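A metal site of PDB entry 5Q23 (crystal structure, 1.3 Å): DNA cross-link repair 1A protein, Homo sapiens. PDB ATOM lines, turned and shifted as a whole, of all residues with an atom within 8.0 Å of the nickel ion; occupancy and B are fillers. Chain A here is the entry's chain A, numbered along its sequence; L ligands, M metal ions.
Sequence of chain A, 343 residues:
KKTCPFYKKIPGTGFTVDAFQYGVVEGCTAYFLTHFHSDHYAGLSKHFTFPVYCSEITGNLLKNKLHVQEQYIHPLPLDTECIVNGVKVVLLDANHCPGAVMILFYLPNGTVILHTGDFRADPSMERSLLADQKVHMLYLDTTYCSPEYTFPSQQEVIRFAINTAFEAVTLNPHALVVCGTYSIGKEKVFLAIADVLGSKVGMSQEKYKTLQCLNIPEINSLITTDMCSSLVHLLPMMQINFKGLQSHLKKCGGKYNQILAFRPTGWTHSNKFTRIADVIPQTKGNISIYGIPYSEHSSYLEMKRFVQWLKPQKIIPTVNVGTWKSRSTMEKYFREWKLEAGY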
ATOM      1  N   ASP A  18       9.166  18.978 -11.790  1.00  0.00           N
ATOM      2  CA  ASP A  18       9.883  19.827 -12.758  1.00  0.00           C
ATOM      3  C   ASP A  18       9.925  19.238 -14.191  1.00  0.00           C
ATOM      4  O   ASP A  18      10.969  19.256 -14.900  1.00  0.00           O
ATOM      5  CB  ASP A  18      11.276  20.206 -12.257  1.00  0.00           C
ATOM      6  CG  ASP A  18      11.239  20.955 -10.920  1.00  0.00           C
ATOM      7  OD1 ASP A  18      10.141  21.403 -10.487  1.00  0.00           O
ATOM      8  OD2 ASP A  18      12.310  21.151 -10.305  1.00  0.00           O
ATOM      9  N   THR A  34       9.174  22.851  -8.232  1.00  0.00           N
ATOM     10  CA  THR A  34       9.941  23.191  -7.026  1.00  0.00           C
ATOM     11  C   THR A  34      10.236  24.708  -6.908  1.00  0.00           C
ATOM     12  O   THR A  34      10.285  25.237  -5.789  1.00  0.00           O
ATOM     13  CB  THR A  34      11.274  22.419  -6.925  1.00  0.00           C
ATOM     14  OG1 THR A  34      12.153  22.746  -8.050  1.00  0.00           O
ATOM     15  CG2 THR A  34      11.018  20.905  -6.872  1.00  0.00           C
ATOM     16  N   HIS A  35      10.444  25.386  -8.054  1.00  0.00           N
ATOM     17  CA  HIS A  35      10.816  26.800  -8.050  1.00  0.00           C
ATOM     18  C   HIS A  35      10.716  27.412  -9.436  1.00  0.00           C
ATOM     19  O   HIS A  35      10.780  26.704 -10.446  1.00  0.00           O
ATOM     20  CB  HIS A  35      12.220  27.045  -7.414  1.00  0.00           C
ATOM     21  CG  HIS A  35      13.397  26.522  -8.180  1.00  0.00           C
ATOM     22  ND1 HIS A  35      13.696  25.184  -8.363  1.00  0.00           N
ATOM     23  CD2 HIS A  35      14.397  27.206  -8.784  1.00  0.00           C
ATOM     24  CE1 HIS A  35      14.825  25.079  -9.048  1.00  0.00           C
ATOM     25  NE2 HIS A  35      15.276  26.287  -9.286  1.00  0.00           N
ATOM     26  N   PHE A  36      10.649  28.751  -9.479  1.00  0.00           N
ATOM     27  CA  PHE A  36      10.503  29.507 -10.742  1.00  0.00           C
ATOM     28  C   PHE A  36      11.847  29.880 -11.369  1.00  0.00           C
ATOM     29  O   PHE A  36      12.186  31.102 -11.434  1.00  0.00           O
ATOM     30  CB  PHE A  36       9.613  30.760 -10.498  1.00  0.00           C
ATOM     31  CG  PHE A  36       9.097  31.431 -11.763  1.00  0.00           C
ATOM     32  CD1 PHE A  36       8.020  30.900 -12.471  1.00  0.00           C
ATOM     33  CD2 PHE A  36       9.654  32.617 -12.225  1.00  0.00           C
ATOM     34  CE1 PHE A  36       7.517  31.531 -13.594  1.00  0.00           C
ATOM     35  CE2 PHE A  36       9.161  33.253 -13.357  1.00  0.00           C
ATOM     36  CZ  PHE A  36       8.113  32.699 -14.046  1.00  0.00           C
ATOM     37  N   HIS A  37      12.602  28.855 -11.806  1.00  0.00           N
ATOM     38  CA  HIS A  37      13.747  28.985 -12.719  1.00  0.00           C
ATOM     39  C   HIS A  37      13.455  28.291 -14.052  1.00  0.00           C
ATOM     40  O   HIS A  37      12.855  27.208 -14.097  1.00  0.00           O
ATOM     41  CB  HIS A  37      15.057  28.475 -12.117  1.00  0.00           C
ATOM     42  CG  HIS A  37      15.705  29.420 -11.118  1.00  0.00           C
ATOM     43  ND1 HIS A  37      16.679  29.003 -10.231  1.00  0.00           N
ATOM     44  CD2 HIS A  37      15.577  30.754 -10.925  1.00  0.00           C
ATOM     45  CE1 HIS A  37      17.107  30.030  -9.511  1.00  0.00           C
ATOM     46  NE2 HIS A  37      16.460  31.108  -9.936  1.00  0.00           N
ATOM     47  N   SER A  38      13.896  28.918 -15.158  1.00  0.00           N
ATOM     48  CA  SER A  38      13.412  28.523 -16.469  1.00  0.00           C
ATOM     49  C   SER A  38      13.770  27.096 -16.885  1.00  0.00           C
ATOM     50  O   SER A  38      12.976  26.471 -17.610  1.00  0.00           O
ATOM     51  CB  SER A  38      13.810  29.564 -17.524  1.00  0.00           C
ATOM     52  OG  SER A  38      15.206  29.666 -17.658  1.00  0.00           O
ATOM     53  N   ASP A  39      14.909  26.553 -16.421  1.00  0.00           N
ATOM     54  CA  ASP A  39      15.243  25.165 -16.734  1.00  0.00           C
ATOM     55  C   ASP A  39      14.228  24.195 -16.079  1.00  0.00           C
ATOM     56  O   ASP A  39      14.061  23.068 -16.553  1.00  0.00           O
ATOM     57  CB  ASP A  39      16.658  24.759 -16.283  1.00  0.00           C
ATOM     58  CG  ASP A  39      17.771  25.170 -17.266  1.00  0.00           C
ATOM     59  OD1 ASP A  39      17.523  25.708 -18.370  1.00  0.00           O
ATOM     60  OD2 ASP A  39      18.951  24.932 -16.904  1.00  0.00           O
ATOM     61  N   HIS A  40      13.578  24.619 -14.987  1.00  0.00           N
ATOM     62  CA  HIS A  40      12.644  23.797 -14.227  1.00  0.00           C
ATOM     63  C   HIS A  40      11.197  23.989 -14.692  1.00  0.00           C
ATOM     64  O   HIS A  40      10.429  22.987 -14.768  1.00  0.00           O
ATOM     65  CB  HIS A  40      12.843  24.068 -12.702  1.00  0.00           C
ATOM     66  CG  HIS A  40      14.208  23.691 -12.244  1.00  0.00           C
ATOM     67  ND1 HIS A  40      14.478  22.507 -11.603  1.00  0.00           N
ATOM     68  CD2 HIS A  40      15.391  24.325 -12.396  1.00  0.00           C
ATOM     69  CE1 HIS A  40      15.780  22.430 -11.377  1.00  0.00           C
ATOM     70  NE2 HIS A  40      16.350  23.521 -11.843  1.00  0.00           N
ATOM     71  N   HIS A  96      17.094  28.377  -1.470  1.00  0.00           N
ATOM     72  CA  HIS A  96      17.532  28.614  -2.866  1.00  0.00           C
ATOM     73  C   HIS A  96      17.090  30.055  -3.239  1.00  0.00           C
ATOM     74  O   HIS A  96      17.612  31.004  -2.592  1.00  0.00           O
ATOM     75  CB  HIS A  96      17.035  27.481  -3.799  1.00  0.00           C
ATOM     76  CG  HIS A  96      17.513  27.544  -5.223  1.00  0.00           C
ATOM     77  ND1 HIS A  96      18.837  27.623  -5.593  1.00  0.00           N
ATOM     78  CD2 HIS A  96      16.816  27.496  -6.389  1.00  0.00           C
ATOM     79  CE1 HIS A  96      18.924  27.669  -6.910  1.00  0.00           C
ATOM     80  NE2 HIS A  96      17.712  27.575  -7.422  1.00  0.00           N
ATOM     81  N   CYS A  97      16.204  30.242  -4.208  1.00  0.00           N
ATOM     82  CA  CYS A  97      15.605  31.541  -4.546  1.00  0.00           C
ATOM     83  C   CYS A  97      14.218  31.692  -3.853  1.00  0.00           C
ATOM     84  O   CYS A  97      13.703  30.716  -3.282  1.00  0.00           O
ATOM     85  CB  CYS A  97      15.454  31.623  -6.076  1.00  0.00           C
ATOM     86  SG  CYS A  97      14.309  30.400  -6.813  1.00  0.00           S
ATOM     87  N   ALA A 100      11.276  28.749  -3.478  1.00  0.00           N
ATOM     88  CA  ALA A 100      11.843  27.421  -3.768  1.00  0.00           C
ATOM     89  C   ALA A 100      11.623  26.472  -2.614  1.00  0.00           C
ATOM     90  O   ALA A 100      11.847  26.830  -1.436  1.00  0.00           O
ATOM     91  CB  ALA A 100      13.337  27.493  -4.086  1.00  0.00           C
ATOM     92  N   GLY A 117      14.667  19.536  -4.875  1.00  0.00           N
ATOM     93  CA  GLY A 117      14.691  20.532  -5.959  1.00  0.00           C
ATOM     94  C   GLY A 117      16.098  21.097  -6.111  1.00  0.00           C
ATOM     95  O   GLY A 117      17.055  20.342  -6.008  1.00  0.00           O
ATOM     96  N   ASP A 118      16.221  22.419  -6.323  1.00  0.00           N
ATOM     97  CA  ASP A 118      17.533  23.125  -6.144  1.00  0.00           C
ATOM     98  C   ASP A 118      17.617  23.622  -4.694  1.00  0.00           C
ATOM     99  O   ASP A 118      16.628  24.154  -4.183  1.00  0.00           O
ATOM    100  CB  ASP A 118      17.696  24.292  -7.116  1.00  0.00           C
ATOM    101  CG  ASP A 118      18.051  23.888  -8.541  1.00  0.00           C
ATOM    102  OD1 ASP A 118      18.389  22.716  -8.845  1.00  0.00           O
ATOM    103  OD2 ASP A 118      18.073  24.838  -9.382  1.00  0.00           O
ATOM    104  N   PHE A 119      18.746  23.410  -4.017  1.00  0.00           N
ATOM    105  CA  PHE A 119      18.876  23.820  -2.587  1.00  0.00           C
ATOM    106  C   PHE A 119      20.311  24.238  -2.249  1.00  0.00           C
ATOM    107  O   PHE A 119      21.257  23.819  -2.929  1.00  0.00           O
ATOM    108  CB  PHE A 119      18.284  22.767  -1.586  1.00  0.00           C
ATOM    109  CG  PHE A 119      19.221  21.618  -1.159  1.00  0.00           C
ATOM    110  CD1 PHE A 119      19.190  21.140   0.142  1.00  0.00           C
ATOM    111  CD2 PHE A 119      20.076  20.945  -2.053  1.00  0.00           C
ATOM    112  CE1 PHE A 119      19.969  20.044   0.553  1.00  0.00           C
ATOM    113  CE2 PHE A 119      20.856  19.863  -1.643  1.00  0.00           C
ATOM    114  CZ  PHE A 119      20.805  19.409  -0.339  1.00  0.00           C
ATOM    115  N   ASP A 141      20.053  17.667  -5.468  1.00  0.00           N
ATOM    116  CA  ASP A 141      20.746  18.708  -6.254  1.00  0.00           C
ATOM    117  C   ASP A 141      22.248  18.579  -6.077  1.00  0.00           C
ATOM    118  O   ASP A 141      22.794  18.965  -5.051  1.00  0.00           O
ATOM    119  CB  ASP A 141      20.267  20.091  -5.792  1.00  0.00           C
ATOM    120  CG  ASP A 141      21.098  21.250  -6.375  1.00  0.00           C
ATOM    121  OD1 ASP A 141      21.859  21.030  -7.345  1.00  0.00           O
ATOM    122  OD2 ASP A 141      20.922  22.382  -5.851  1.00  0.00           O
ATOM    123  N   THR A 143      24.602  19.935  -8.184  1.00  0.00           N
ATOM    124  CA  THR A 143      25.265  20.953  -9.012  1.00  0.00           C
ATOM    125  C   THR A 143      26.792  21.056  -8.743  1.00  0.00           C
ATOM    126  O   THR A 143      27.596  20.974  -9.716  1.00  0.00           O
ATOM    127  CB  THR A 143      24.610  22.346  -8.799  1.00  0.00           C
ATOM    128  OG1 THR A 143      23.225  22.346  -9.192  1.00  0.00           O
ATOM    129  CG2 THR A 143      25.331  23.435  -9.628  1.00  0.00           C
ATOM    130  N   SER A 183      17.233  36.287 -13.583  1.00  0.00           N
ATOM    131  CA  SER A 183      16.281  35.358 -13.005  1.00  0.00           C
ATOM    132  C   SER A 183      16.022  35.849 -11.586  1.00  0.00           C
ATOM    133  O   SER A 183      16.729  36.755 -11.095  1.00  0.00           O
ATOM    134  CB  SER A 183      16.849  33.923 -12.909  1.00  0.00           C
ATOM    135  OG  SER A 183      18.013  33.927 -12.084  1.00  0.00           O
ATOM    136  N   ILE A 184      15.060  35.257 -10.908  1.00  0.00           N
ATOM    137  CA  ILE A 184      14.891  35.480  -9.482  1.00  0.00           C
ATOM    138  C   ILE A 184      16.026  34.777  -8.708  1.00  0.00           C
ATOM    139  O   ILE A 184      16.717  33.884  -9.238  1.00  0.00           O
ATOM    140  CB  ILE A 184      13.494  35.066  -8.940  1.00  0.00           C
ATOM    141  CG1 ILE A 184      13.252  33.562  -9.020  1.00  0.00           C
ATOM    142  CG2 ILE A 184      12.402  35.825  -9.685  1.00  0.00           C
ATOM    143  CD1 ILE A 184      12.071  33.086  -8.204  1.00  0.00           C
ATOM    144  N   GLU A 296      23.521  30.165  -4.483  1.00  0.00           N
ATOM    145  CA  GLU A 296      22.269  29.605  -3.934  1.00  0.00           C
ATOM    146  C   GLU A 296      22.196  28.073  -4.122  1.00  0.00           C
ATOM    147  O   GLU A 296      21.092  27.460  -4.062  1.00  0.00           O
ATOM    148  CB  GLU A 296      21.050  30.363  -4.475  1.00  0.00           C
ATOM    149  CG  GLU A 296      20.964  31.808  -3.890  1.00  0.00           C
ATOM    150  CD  GLU A 296      19.690  32.620  -4.234  1.00  0.00           C
ATOM    151  OE1 GLU A 296      18.989  32.264  -5.230  1.00  0.00           O
ATOM    152  OE2 GLU A 296      19.421  33.634  -3.544  1.00  0.00           O
ATOM    153  N   HIS A 297      23.353  27.444  -4.352  1.00  0.00           N
ATOM    154  CA  HIS A 297      23.451  25.973  -4.304  1.00  0.00           C
ATOM    155  C   HIS A 297      24.481  25.554  -3.222  1.00  0.00           C
ATOM    156  O   HIS A 297      25.457  26.283  -2.901  1.00  0.00           O
ATOM    157  CB  HIS A 297      23.934  25.392  -5.659  1.00  0.00           C
ATOM    158  CG  HIS A 297      22.987  25.555  -6.810  1.00  0.00           C
ATOM    159  ND1 HIS A 297      21.961  24.678  -7.096  1.00  0.00           N
ATOM    160  CD2 HIS A 297      22.961  26.478  -7.789  1.00  0.00           C
ATOM    161  CE1 HIS A 297      21.337  25.076  -8.194  1.00  0.00           C
ATOM    162  NE2 HIS A 297      21.933  26.165  -8.645  1.00  0.00           N
HETATM  163  C1  LIG L   1      19.386  27.860 -12.282  1.00  0.00           C
HETATM  164  C2  LIG L   1      20.151  27.673 -10.985  1.00  0.00           C
HETATM  165  C3  LIG L   1      18.432  26.704 -12.553  1.00  0.00           C
HETATM  166  O1  LIG L   1      21.389  27.748 -10.918  1.00  0.00           O
HETATM  167  O2  LIG L   1      19.504  27.463  -9.959  1.00  0.00           O
HETATM  168  O3  LIG L   1      18.515  26.138 -13.664  1.00  0.00           O
HETATM  169  O4  LIG L   1      17.576  26.397 -11.684  1.00  0.00           O
HETATM  170 NI    NI M   1      17.435  26.925  -9.663  1.00  0.00          NI
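Along chain A the residues within 4 Å of the nickel ion span positions 35 to 118.
The nickel ion is bound by O4 of the ligand (2.1 Å). O2 of the ligand is bound to the nickel ion (2.2 Å). OD2 of Asp 118 binds the nickel ion, at 2.2 Å. The nickel ion is bound by a ring nitrogen (ND1) of His 37, at 2.3 Å. A ring nitrogen (NE2) of His 35 binds the nickel ion (2.3 Å). A ring nitrogen (NE2) of His 96 is bound to the nickel ion, at 2.3 Å. The nickel ion has six donor atoms within binding distance.
OD2 of Asp 118 lies close to NE2 of His 40 (3.3 Å). A ring nitrogen (NE2) of His 37 is in hydrogen-bond range of the backbone carbonyl oxygen (O) of Ile 184, at 2.9 Å. A ring nitrogen (ND1) of His 35 is in hydrogen-bond range of the side-chain hydroxyl of Thr 34 (2.9 Å). The backbone carbonyl oxygen (O) of Glu 296 is in hydrogen-bond range of a ring nitrogen (ND1) of His 96.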
